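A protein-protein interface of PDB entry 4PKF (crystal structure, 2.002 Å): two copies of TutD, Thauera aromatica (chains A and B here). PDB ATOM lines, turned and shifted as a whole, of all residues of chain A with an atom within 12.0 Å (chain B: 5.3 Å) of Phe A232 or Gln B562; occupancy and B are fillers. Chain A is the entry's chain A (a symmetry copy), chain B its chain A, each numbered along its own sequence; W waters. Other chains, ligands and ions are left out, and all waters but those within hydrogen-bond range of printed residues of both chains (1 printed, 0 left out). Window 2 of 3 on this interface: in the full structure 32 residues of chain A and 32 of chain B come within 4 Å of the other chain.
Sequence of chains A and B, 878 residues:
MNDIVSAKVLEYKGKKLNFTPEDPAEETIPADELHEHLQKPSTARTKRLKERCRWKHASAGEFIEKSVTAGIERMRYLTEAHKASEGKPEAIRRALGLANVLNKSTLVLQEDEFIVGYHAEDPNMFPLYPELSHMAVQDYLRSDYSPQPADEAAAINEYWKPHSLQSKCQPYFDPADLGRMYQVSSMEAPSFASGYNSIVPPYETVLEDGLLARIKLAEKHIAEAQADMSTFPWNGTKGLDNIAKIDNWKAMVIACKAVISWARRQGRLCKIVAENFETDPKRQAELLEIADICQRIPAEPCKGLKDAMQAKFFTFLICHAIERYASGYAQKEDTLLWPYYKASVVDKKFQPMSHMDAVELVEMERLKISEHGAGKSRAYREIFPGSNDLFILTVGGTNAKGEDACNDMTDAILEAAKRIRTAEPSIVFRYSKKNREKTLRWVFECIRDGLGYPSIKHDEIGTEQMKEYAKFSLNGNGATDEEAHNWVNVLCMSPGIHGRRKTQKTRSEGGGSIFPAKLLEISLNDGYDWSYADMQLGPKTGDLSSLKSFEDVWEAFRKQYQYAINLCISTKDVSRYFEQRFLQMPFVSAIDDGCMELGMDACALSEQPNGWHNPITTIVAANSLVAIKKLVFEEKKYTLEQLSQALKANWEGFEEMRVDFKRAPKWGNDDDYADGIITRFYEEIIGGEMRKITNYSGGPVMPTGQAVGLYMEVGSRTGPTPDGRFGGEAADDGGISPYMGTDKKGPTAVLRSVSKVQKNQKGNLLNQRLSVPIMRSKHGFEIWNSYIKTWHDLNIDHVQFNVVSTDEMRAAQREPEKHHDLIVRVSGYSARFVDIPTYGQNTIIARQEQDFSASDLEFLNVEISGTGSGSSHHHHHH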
ATOM      1  N   GLU A 224     -11.618  33.003 -16.688  1.00  0.00           N
ATOM      2  CA  GLU A 224     -12.927  32.598 -17.181  1.00  0.00           C
ATOM      3  C   GLU A 224     -12.987  32.369 -18.701  1.00  0.00           C
ATOM      4  O   GLU A 224     -13.625  31.417 -19.184  1.00  0.00           O
ATOM      5  CB  GLU A 224     -13.961  33.622 -16.787  1.00  0.00           C
ATOM      6  CG  GLU A 224     -14.339  33.481 -15.320  1.00  0.00           C
ATOM      7  CD  GLU A 224     -15.312  34.554 -14.823  1.00  0.00           C
ATOM      8  OE1 GLU A 224     -15.755  35.412 -15.634  1.00  0.00           O
ATOM      9  OE2 GLU A 224     -15.620  34.519 -13.603  1.00  0.00           O
ATOM     10  N   ALA A 225     -12.354  33.257 -19.450  1.00  0.00           N
ATOM     11  CA  ALA A 225     -12.317  33.107 -20.904  1.00  0.00           C
ATOM     12  C   ALA A 225     -11.544  31.824 -21.315  1.00  0.00           C
ATOM     13  O   ALA A 225     -12.007  31.068 -22.193  1.00  0.00           O
ATOM     14  CB  ALA A 225     -11.714  34.363 -21.543  1.00  0.00           C
ATOM     15  N   GLN A 226     -10.406  31.548 -20.667  1.00  0.00           N
ATOM     16  CA  GLN A 226      -9.660  30.322 -20.979  1.00  0.00           C
ATOM     17  C   GLN A 226     -10.471  29.070 -20.602  1.00  0.00           C
ATOM     18  O   GLN A 226     -10.458  28.077 -21.342  1.00  0.00           O
ATOM     19  CB  GLN A 226      -8.291  30.310 -20.286  1.00  0.00           C
ATOM     20  CG  GLN A 226      -7.398  31.484 -20.728  1.00  0.00           C
ATOM     21  CD  GLN A 226      -6.181  31.621 -19.865  1.00  0.00           C
ATOM     22  OE1 GLN A 226      -6.230  31.347 -18.665  1.00  0.00           O
ATOM     23  NE2 GLN A 226      -5.069  32.023 -20.462  1.00  0.00           N
ATOM     24  N   ALA A 227     -11.207  29.136 -19.495  1.00  0.00           N
ATOM     25  CA  ALA A 227     -12.102  28.042 -19.108  1.00  0.00           C
ATOM     26  C   ALA A 227     -13.185  27.855 -20.159  1.00  0.00           C
ATOM     27  O   ALA A 227     -13.521  26.724 -20.508  1.00  0.00           O
ATOM     28  CB  ALA A 227     -12.733  28.303 -17.750  1.00  0.00           C
ATOM     29  N   ASP A 228     -13.729  28.965 -20.647  1.00  0.00           N
ATOM     30  CA  ASP A 228     -14.765  28.947 -21.679  1.00  0.00           C
ATOM     31  C   ASP A 228     -14.274  28.220 -22.940  1.00  0.00           C
ATOM     32  O   ASP A 228     -15.006  27.463 -23.565  1.00  0.00           O
ATOM     33  CB  ASP A 228     -15.202  30.387 -22.041  1.00  0.00           C
ATOM     34  CG  ASP A 228     -16.389  30.418 -23.034  1.00  0.00           C
ATOM     35  OD1 ASP A 228     -17.395  29.736 -22.768  1.00  0.00           O
ATOM     36  OD2 ASP A 228     -16.333  31.118 -24.086  1.00  0.00           O
ATOM     37  N   MET A 229     -13.021  28.445 -23.287  1.00  0.00           N
ATOM     38  CA  MET A 229     -12.472  27.915 -24.519  1.00  0.00           C
ATOM     39  C   MET A 229     -12.188  26.408 -24.409  1.00  0.00           C
ATOM     40  O   MET A 229     -12.085  25.704 -25.414  1.00  0.00           O
ATOM     41  CB  MET A 229     -11.212  28.698 -24.881  1.00  0.00           C
ATOM     42  CG  MET A 229     -11.507  30.149 -25.418  1.00  0.00           C
ATOM     43  SD  MET A 229      -9.979  30.870 -26.021  1.00  0.00           S
ATOM     44  CE  MET A 229      -9.759  29.960 -27.575  1.00  0.00           C
ATOM     45  N   SER A 230     -12.071  25.901 -23.195  1.00  0.00           N
ATOM     46  CA  SER A 230     -11.817  24.467 -23.049  1.00  0.00           C
ATOM     47  C   SER A 230     -13.078  23.702 -22.646  1.00  0.00           C
ATOM     48  O   SER A 230     -13.014  22.515 -22.353  1.00  0.00           O
ATOM     49  CB  SER A 230     -10.709  24.208 -22.034  1.00  0.00           C
ATOM     50  OG  SER A 230     -11.163  24.638 -20.781  1.00  0.00           O
ATOM     51  N   THR A 231     -14.233  24.359 -22.674  1.00  0.00           N
ATOM     52  CA  THR A 231     -15.465  23.673 -22.295  1.00  0.00           C
ATOM     53  C   THR A 231     -16.107  22.875 -23.443  1.00  0.00           C
ATOM     54  O   THR A 231     -16.325  23.418 -24.530  1.00  0.00           O
ATOM     55  CB  THR A 231     -16.499  24.685 -21.750  1.00  0.00           C
ATOM     56  OG1 THR A 231     -15.976  25.280 -20.549  1.00  0.00           O
ATOM     57  CG2 THR A 231     -17.822  23.970 -21.446  1.00  0.00           C
ATOM     58  N   PHE A 232     -16.405  21.592 -23.204  1.00  0.00           N
ATOM     59  CA  PHE A 232     -17.103  20.769 -24.197  1.00  0.00           C
ATOM     60  C   PHE A 232     -18.581  21.057 -24.100  1.00  0.00           C
ATOM     61  O   PHE A 232     -19.114  21.046 -23.006  1.00  0.00           O
ATOM     62  CB  PHE A 232     -16.855  19.261 -23.980  1.00  0.00           C
ATOM     63  CG  PHE A 232     -17.623  18.370 -24.940  1.00  0.00           C
ATOM     64  CD1 PHE A 232     -18.866  17.859 -24.598  1.00  0.00           C
ATOM     65  CD2 PHE A 232     -17.102  18.051 -26.200  1.00  0.00           C
ATOM     66  CE1 PHE A 232     -19.588  17.035 -25.483  1.00  0.00           C
ATOM     67  CE2 PHE A 232     -17.813  17.248 -27.096  1.00  0.00           C
ATOM     68  CZ  PHE A 232     -19.067  16.717 -26.737  1.00  0.00           C
ATOM     69  N   PRO A 233     -19.268  21.247 -25.235  1.00  0.00           N
ATOM     70  CA  PRO A 233     -18.804  21.242 -26.633  1.00  0.00           C
ATOM     71  C   PRO A 233     -18.446  22.625 -27.143  1.00  0.00           C
ATOM     72  O   PRO A 233     -19.219  23.583 -26.974  1.00  0.00           O
ATOM     73  CB  PRO A 233     -20.011  20.701 -27.408  1.00  0.00           C
ATOM     74  CG  PRO A 233     -21.188  21.174 -26.581  1.00  0.00           C
ATOM     75  CD  PRO A 233     -20.739  21.185 -25.140  1.00  0.00           C
ATOM     76  N   TRP A 234     -17.283  22.718 -27.772  1.00  0.00           N
ATOM     77  CA  TRP A 234     -16.836  23.970 -28.404  1.00  0.00           C
ATOM     78  C   TRP A 234     -17.836  24.476 -29.445  1.00  0.00           C
ATOM     79  O   TRP A 234     -18.477  23.681 -30.165  1.00  0.00           O
ATOM     80  CB  TRP A 234     -15.460  23.729 -29.059  1.00  0.00           C
ATOM     81  CG  TRP A 234     -14.945  24.781 -30.023  1.00  0.00           C
ATOM     82  CD1 TRP A 234     -15.031  24.773 -31.413  1.00  0.00           C
ATOM     83  CD2 TRP A 234     -14.181  25.939 -29.672  1.00  0.00           C
ATOM     84  NE1 TRP A 234     -14.396  25.900 -31.929  1.00  0.00           N
ATOM     85  CE2 TRP A 234     -13.858  26.620 -30.886  1.00  0.00           C
ATOM     86  CE3 TRP A 234     -13.741  26.476 -28.447  1.00  0.00           C
ATOM     87  CZ2 TRP A 234     -13.128  27.800 -30.900  1.00  0.00           C
ATOM     88  CZ3 TRP A 234     -12.994  27.633 -28.470  1.00  0.00           C
ATOM     89  CH2 TRP A 234     -12.712  28.303 -29.692  1.00  0.00           C
ATOM     90  N   ASN A 235     -17.950  25.803 -29.523  1.00  0.00           N
ATOM     91  CA  ASN A 235     -18.725  26.460 -30.569  1.00  0.00           C
ATOM     92  C   ASN A 235     -17.850  27.530 -31.187  1.00  0.00           C
ATOM     93  O   ASN A 235     -17.630  28.593 -30.579  1.00  0.00           O
ATOM     94  CB  ASN A 235     -20.013  27.093 -30.018  1.00  0.00           C
ATOM     95  CG  ASN A 235     -20.872  27.696 -31.115  1.00  0.00           C
ATOM     96  OD1 ASN A 235     -20.376  28.085 -32.189  1.00  0.00           O
ATOM     97  ND2 ASN A 235     -22.175  27.747 -30.874  1.00  0.00           N
ATOM     98  N   GLY A 236     -17.371  27.267 -32.400  1.00  0.00           N
ATOM     99  CA  GLY A 236     -16.438  28.182 -33.043  1.00  0.00           C
ATOM    100  C   GLY A 236     -16.974  29.527 -33.484  1.00  0.00           C
ATOM    101  O   GLY A 236     -16.189  30.416 -33.831  1.00  0.00           O
ATOM    102  N   LYS A 238     -18.585  31.352 -31.378  1.00  0.00           N
ATOM    103  CA  LYS A 238     -18.565  32.094 -30.122  1.00  0.00           C
ATOM    104  C   LYS A 238     -17.185  32.097 -29.479  1.00  0.00           C
ATOM    105  O   LYS A 238     -16.718  33.116 -28.978  1.00  0.00           O
ATOM    106  CB  LYS A 238     -19.563  31.491 -29.122  1.00  0.00           C
ATOM    107  CG  LYS A 238     -20.998  31.530 -29.597  1.00  0.00           C
ATOM    108  CD  LYS A 238     -21.937  31.042 -28.500  1.00  0.00           C
ATOM    109  CE  LYS A 238     -23.381  31.234 -28.949  1.00  0.00           C
ATOM    110  NZ  LYS A 238     -24.374  30.961 -27.873  1.00  0.00           N
ATOM    111  N   GLY A 239     -16.531  30.940 -29.477  1.00  0.00           N
ATOM    112  CA  GLY A 239     -15.377  30.764 -28.614  1.00  0.00           C
ATOM    113  C   GLY A 239     -14.187  31.584 -29.086  1.00  0.00           C
ATOM    114  O   GLY A 239     -13.279  31.872 -28.321  1.00  0.00           O
ATOM    115  N   ASN A 242     -13.058  35.038 -27.610  1.00  0.00           N
ATOM    116  CA  ASN A 242     -12.210  35.103 -26.416  1.00  0.00           C
ATOM    117  C   ASN A 242     -10.784  35.545 -26.746  1.00  0.00           C
ATOM    118  O   ASN A 242     -10.055  36.009 -25.872  1.00  0.00           O
ATOM    119  CB  ASN A 242     -12.193  33.725 -25.718  1.00  0.00           C
ATOM    120  CG  ASN A 242     -13.501  33.421 -25.006  1.00  0.00           C
ATOM    121  OD1 ASN A 242     -13.965  34.215 -24.211  1.00  0.00           O
ATOM    122  ND2 ASN A 242     -14.143  32.338 -25.375  1.00  0.00           N
ATOM    123  N   PHE B 557     -14.414   6.157 -21.695  1.00  0.00           N
ATOM    124  CA  PHE B 557     -14.019   6.395 -23.063  1.00  0.00           C
ATOM    125  C   PHE B 557     -14.700   7.686 -23.559  1.00  0.00           C
ATOM    126  O   PHE B 557     -14.068   8.523 -24.191  1.00  0.00           O
ATOM    127  CB  PHE B 557     -14.372   5.251 -23.999  1.00  0.00           C
ATOM    128  CG  PHE B 557     -13.998   5.555 -25.424  1.00  0.00           C
ATOM    129  CD1 PHE B 557     -14.840   6.310 -26.233  1.00  0.00           C
ATOM    130  CD2 PHE B 557     -12.761   5.174 -25.919  1.00  0.00           C
ATOM    131  CE1 PHE B 557     -14.471   6.657 -27.534  1.00  0.00           C
ATOM    132  CE2 PHE B 557     -12.386   5.502 -27.217  1.00  0.00           C
ATOM    133  CZ  PHE B 557     -13.232   6.242 -28.021  1.00  0.00           C
ATOM    134  N   ARG B 558     -15.994   7.815 -23.289  1.00  0.00           N
ATOM    135  CA  ARG B 558     -16.732   9.011 -23.693  1.00  0.00           C
ATOM    136  C   ARG B 558     -16.021  10.286 -23.274  1.00  0.00           C
ATOM    137  O   ARG B 558     -15.858  11.209 -24.086  1.00  0.00           O
ATOM    138  CB  ARG B 558     -18.146   9.008 -23.133  1.00  0.00           C
ATOM    139  CG  ARG B 558     -18.998  10.138 -23.784  1.00  0.00           C
ATOM    140  CD  ARG B 558     -20.236  10.501 -22.933  1.00  0.00           C
ATOM    141  NE  ARG B 558     -21.077   9.361 -22.608  1.00  0.00           N
ATOM    142  CZ  ARG B 558     -21.882   8.734 -23.463  1.00  0.00           C
ATOM    143  NH1 ARG B 558     -22.604   7.716 -23.028  1.00  0.00           N
ATOM    144  NH2 ARG B 558     -21.990   9.124 -24.731  1.00  0.00           N
ATOM    145  N   LYS B 559     -15.586  10.347 -22.015  1.00  0.00           N
ATOM    146  CA  LYS B 559     -14.935  11.540 -21.518  1.00  0.00           C
ATOM    147  C   LYS B 559     -13.571  11.793 -22.163  1.00  0.00           C
ATOM    148  O   LYS B 559     -13.222  12.941 -22.461  1.00  0.00           O
ATOM    149  CB  LYS B 559     -14.786  11.476 -19.999  1.00  0.00           C
ATOM    150  CG  LYS B 559     -16.067  11.808 -19.227  1.00  0.00           C
ATOM    151  CD  LYS B 559     -15.849  11.582 -17.727  1.00  0.00           C
ATOM    152  CE  LYS B 559     -17.130  11.736 -16.910  1.00  0.00           C
ATOM    153  NZ  LYS B 559     -17.058  10.850 -15.715  1.00  0.00           N
ATOM    154  N   GLN B 560     -12.814  10.730 -22.395  1.00  0.00           N
ATOM    155  CA  GLN B 560     -11.531  10.825 -23.090  1.00  0.00           C
ATOM    156  C   GLN B 560     -11.760  11.417 -24.503  1.00  0.00           C
ATOM    157  O   GLN B 560     -11.052  12.294 -24.940  1.00  0.00           O
ATOM    158  CB  GLN B 560     -10.873   9.430 -23.168  1.00  0.00           C
ATOM    159  CG  GLN B 560     -10.371   8.884 -21.826  1.00  0.00           C
ATOM    160  CD  GLN B 560      -9.250   9.744 -21.268  1.00  0.00           C
ATOM    161  OE1 GLN B 560      -8.582  10.443 -22.023  1.00  0.00           O
ATOM    162  NE2 GLN B 560      -9.033   9.693 -19.955  1.00  0.00           N
ATOM    163  N   TYR B 561     -12.817  10.960 -25.147  1.00  0.00           N
ATOM    164  CA  TYR B 561     -13.161  11.332 -26.512  1.00  0.00           C
ATOM    165  C   TYR B 561     -13.634  12.767 -26.542  1.00  0.00           C
ATOM    166  O   TYR B 561     -13.227  13.532 -27.410  1.00  0.00           O
ATOM    167  CB  TYR B 561     -14.242  10.383 -27.055  1.00  0.00           C
ATOM    168  CG  TYR B 561     -14.539  10.560 -28.525  1.00  0.00           C
ATOM    169  CD1 TYR B 561     -13.641  10.123 -29.486  1.00  0.00           C
ATOM    170  CD2 TYR B 561     -15.717  11.176 -28.956  1.00  0.00           C
ATOM    171  CE1 TYR B 561     -13.917  10.270 -30.849  1.00  0.00           C
ATOM    172  CE2 TYR B 561     -15.999  11.319 -30.303  1.00  0.00           C
ATOM    173  CZ  TYR B 561     -15.088  10.868 -31.243  1.00  0.00           C
ATOM    174  OH  TYR B 561     -15.363  10.998 -32.586  1.00  0.00           O
ATOM    175  N   GLN B 562     -14.437  13.156 -25.552  1.00  0.00           N
ATOM    176  CA  GLN B 562     -14.932  14.535 -25.492  1.00  0.00           C
ATOM    177  C   GLN B 562     -13.780  15.513 -25.289  1.00  0.00           C
ATOM    178  O   GLN B 562     -13.701  16.525 -25.959  1.00  0.00           O
ATOM    179  CB  GLN B 562     -15.970  14.703 -24.372  1.00  0.00           C
ATOM    180  CG  GLN B 562     -17.358  14.137 -24.692  1.00  0.00           C
ATOM    181  CD  GLN B 562     -18.246  14.097 -23.461  1.00  0.00           C
ATOM    182  OE1 GLN B 562     -17.757  14.159 -22.329  1.00  0.00           O
ATOM    183  NE2 GLN B 562     -19.545  13.971 -23.672  1.00  0.00           N
ATOM    184  N   TYR B 563     -12.880  15.197 -24.371  1.00  0.00           N
ATOM    185  CA  TYR B 563     -11.715  16.046 -24.137  1.00  0.00           C
ATOM    186  C   TYR B 563     -10.889  16.189 -25.416  1.00  0.00           C
ATOM    187  O   TYR B 563     -10.460  17.290 -25.767  1.00  0.00           O
ATOM    188  CB  TYR B 563     -10.847  15.475 -22.996  1.00  0.00           C
ATOM    189  CG  TYR B 563      -9.454  16.071 -22.952  1.00  0.00           C
ATOM    190  CD1 TYR B 563      -8.424  15.488 -23.678  1.00  0.00           C
ATOM    191  CD2 TYR B 563      -9.164  17.174 -22.169  1.00  0.00           C
ATOM    192  CE1 TYR B 563      -7.157  15.989 -23.654  1.00  0.00           C
ATOM    193  CE2 TYR B 563      -7.876  17.712 -22.149  1.00  0.00           C
ATOM    194  CZ  TYR B 563      -6.880  17.103 -22.915  1.00  0.00           C
ATOM    195  OH  TYR B 563      -5.571  17.566 -22.949  1.00  0.00           O
ATOM    196  N   ALA B 564     -10.657  15.064 -26.099  1.00  0.00           N
ATOM    197  CA  ALA B 564      -9.810  15.065 -27.287  1.00  0.00           C
ATOM    198  C   ALA B 564     -10.468  15.808 -28.460  1.00  0.00           C
ATOM    199  O   ALA B 564      -9.828  16.638 -29.135  1.00  0.00           O
ATOM    200  CB  ALA B 564      -9.462  13.612 -27.689  1.00  0.00           C
ATOM    201  N   ILE B 565     -11.732  15.496 -28.739  1.00  0.00           N
ATOM    202  CA  ILE B 565     -12.367  16.094 -29.916  1.00  0.00           C
ATOM    203  C   ILE B 565     -12.552  17.611 -29.717  1.00  0.00           C
ATOM    204  O   ILE B 565     -12.491  18.352 -30.673  1.00  0.00           O
ATOM    205  CB  ILE B 565     -13.719  15.407 -30.247  1.00  0.00           C
ATOM    206  CG1 ILE B 565     -14.219  15.824 -31.649  1.00  0.00           C
ATOM    207  CG2 ILE B 565     -14.786  15.703 -29.171  1.00  0.00           C
ATOM    208  CD1 ILE B 565     -13.319  15.380 -32.812  1.00  0.00           C
ATOM    209  N   ASN B 566     -12.734  18.075 -28.478  1.00  0.00           N
ATOM    210  CA  ASN B 566     -12.845  19.509 -28.257  1.00  0.00           C
ATOM    211  C   ASN B 566     -11.557  20.225 -28.653  1.00  0.00           C
ATOM    212  O   ASN B 566     -11.618  21.264 -29.263  1.00  0.00           O
ATOM    213  CB  ASN B 566     -13.198  19.822 -26.776  1.00  0.00           C
ATOM    214  CG  ASN B 566     -14.236  20.960 -26.649  1.00  0.00           C
ATOM    215  OD1 ASN B 566     -15.373  20.833 -27.131  1.00  0.00           O
ATOM    216  ND2 ASN B 566     -13.824  22.087 -26.065  1.00  0.00           N
ATOM    217  N   LEU B 567     -10.396  19.679 -28.290  1.00  0.00           N
ATOM    218  CA  LEU B 567      -9.110  20.251 -28.678  1.00  0.00           C
ATOM    219  C   LEU B 567      -8.903  20.204 -30.176  1.00  0.00           C
ATOM    220  O   LEU B 567      -8.435  21.179 -30.804  1.00  0.00           O
ATOM    221  CB  LEU B 567      -7.962  19.496 -27.989  1.00  0.00           C
ATOM    222  CG  LEU B 567      -7.709  19.876 -26.538  1.00  0.00           C
ATOM    223  CD1 LEU B 567      -6.694  18.892 -25.865  1.00  0.00           C
ATOM    224  CD2 LEU B 567      -7.228  21.296 -26.475  1.00  0.00           C
ATOM    225  N   GLU B 689     -21.194  12.437 -30.190  1.00  0.00           N
ATOM    226  CA  GLU B 689     -20.523  13.448 -29.368  1.00  0.00           C
ATOM    227  C   GLU B 689     -19.891  14.525 -30.242  1.00  0.00           C
ATOM    228  O   GLU B 689     -19.889  15.714 -29.894  1.00  0.00           O
ATOM    229  CB  GLU B 689     -19.455  12.819 -28.458  1.00  0.00           C
ATOM    230  CG  GLU B 689     -20.021  11.815 -27.452  1.00  0.00           C
ATOM    231  CD  GLU B 689     -20.942  12.453 -26.413  1.00  0.00           C
ATOM    232  OE1 GLU B 689     -20.805  13.668 -26.180  1.00  0.00           O
ATOM    233  OE2 GLU B 689     -21.778  11.738 -25.811  1.00  0.00           O
ATOM    234  N   LYS B 692     -22.072  17.491 -31.513  1.00  0.00           N
ATOM    235  CA  LYS B 692     -22.405  18.540 -30.551  1.00  0.00           C
ATOM    236  C   LYS B 692     -21.550  19.785 -30.752  1.00  0.00           C
ATOM    237  O   LYS B 692     -21.895  20.869 -30.292  1.00  0.00           O
ATOM    238  CB  LYS B 692     -22.224  18.033 -29.128  1.00  0.00           C
ATOM    239  CG  LYS B 692     -23.133  16.868 -28.798  1.00  0.00           C
ATOM    240  CD  LYS B 692     -22.871  16.380 -27.393  1.00  0.00           C
ATOM    241  CE  LYS B 692     -23.723  15.164 -27.018  1.00  0.00           C
ATOM    242  NZ  LYS B 692     -23.364  14.769 -25.611  1.00  0.00           N
ATOM    243  N   ILE B 693     -20.421  19.625 -31.420  1.00  0.00           N
ATOM    244  CA  ILE B 693     -19.514  20.754 -31.630  1.00  0.00           C
ATOM    245  C   ILE B 693     -19.898  21.491 -32.908  1.00  0.00           C
ATOM    246  O   ILE B 693     -20.268  20.862 -33.901  1.00  0.00           O
ATOM    247  CB  ILE B 693     -18.042  20.300 -31.712  1.00  0.00           C
ATOM    248  CG1 ILE B 693     -17.578  19.761 -30.339  1.00  0.00           C
ATOM    249  CG2 ILE B 693     -17.122  21.439 -32.194  1.00  0.00           C
ATOM    250  CD1 ILE B 693     -16.190  19.045 -30.392  1.00  0.00           C
HETATM  251  O   HOH W   1     -21.582  23.584 -30.151  1.00  0.00           O
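The side-chain amide oxygen (OD1) of Asn B566 sits at hydrogen-bond distance from the backbone NH (N) of Trp A234.
ND2 of Asn B566 lies within hydrogen-bond range of O of Thr A231 (3.2 Å).
The backbone carbonyl oxygen of Ala A227 sits at hydrogen-bond distance from the side-chain hydroxyl of Thr A231 (2.8 Å).
NE2 of Gln B562 sits at hydrogen-bond distance from OE1 of Glu B689 (2.8 Å).
The backbone carbonyl oxygen of Ala A227 sits at hydrogen-bond distance from the side-chain hydroxyl of Ser A230 (3.2 Å).
The guanidinium group (NH2) of Arg B558 lies within salt-bridge range of the side-chain carboxylate (OE2) of Glu B689 (2.8 Å).
OE1 of Glu B689 lies within salt-bridge range of NZ of Lys B692, 2.8 Å away.
Asn B566 touches Ser A230 (ND2 to O, 3.8 Å).
NE2 of Gln B562 touches CE1 of Phe A232, at 3.6 Å.
CG2 of Ile B565 touches CE2 of Phe A232, 3.98 Å away.
Asn B566 touches Phe A232 (OD1 to CD2, 3.4 Å).
O of Glu B689 touches CZ of Phe A232 (3.4 Å).
Phe A232 touches Lys B692.
Pro A233 touches Asn B566 (CA to OD1, 3.5 Å).
O of Lys B692 touches CB of Pro A233 (3.4 Å).
CG1 of Ile B693 touches CB of Pro A233, at 3.9 Å.
Trp A234 touches Ile B693 (O to CG2, 3.3 Å).
Asp A228 touches none of the printed residues of chain B.
Printed residues of chain B within 4 Å of Ser A230: Asn B566.
Of the printed residues of chain B, Thr A231 touches Asn B566 (3.2 Å).
Of the printed residues of chain B, Phe A232 touches Gln B562, Ile B565, Asn B566, Glu B689 and Lys B692.
Printed residues of chain B within 4 Å of Trp A234: Asn B566 (2.8 Å) and Ile B693 (3.3 Å).
No residue of chain A comes within 4 Å of Lys B559.
No residue of chain A comes within 4 Å of Tyr B561.
Of the printed residues of chain A, Gln B562 touches Phe A232 (3.6 Å).
No residue of chain A comes within 4 Å of Ala B564.
Of the printed residues of chain A, Ile B565 touches Phe A232 (3.98 Å).
Of chain A, only Ser A230 (3.8 Å), Thr A231 (3.2 Å), Phe A232 (3.4 Å), Pro A233 (3.5 Å) and Trp A234 (2.8 Å) come within 4 Å of Asn B566.
Leu B567 touches none of the printed residues of chain A.
The nearest printed residue of chain B that does not touch Phe A232 is Ile B693 (4.1 Å).
Hydrophobic or aromatic side chains of chain B that line the printed part of chain A: Ile B565 and Ile B693.
Hydrophobic or aromatic side chains of chain A that line the printed part of chain B: Phe A232, Pro A233 and Trp A234.
No position is printed for both chains.
Water W1 lies within hydrogen-bond range of the backbone carbonyl oxygen of Lys B692 and the backbone carbonyl oxygen of Trp A234.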
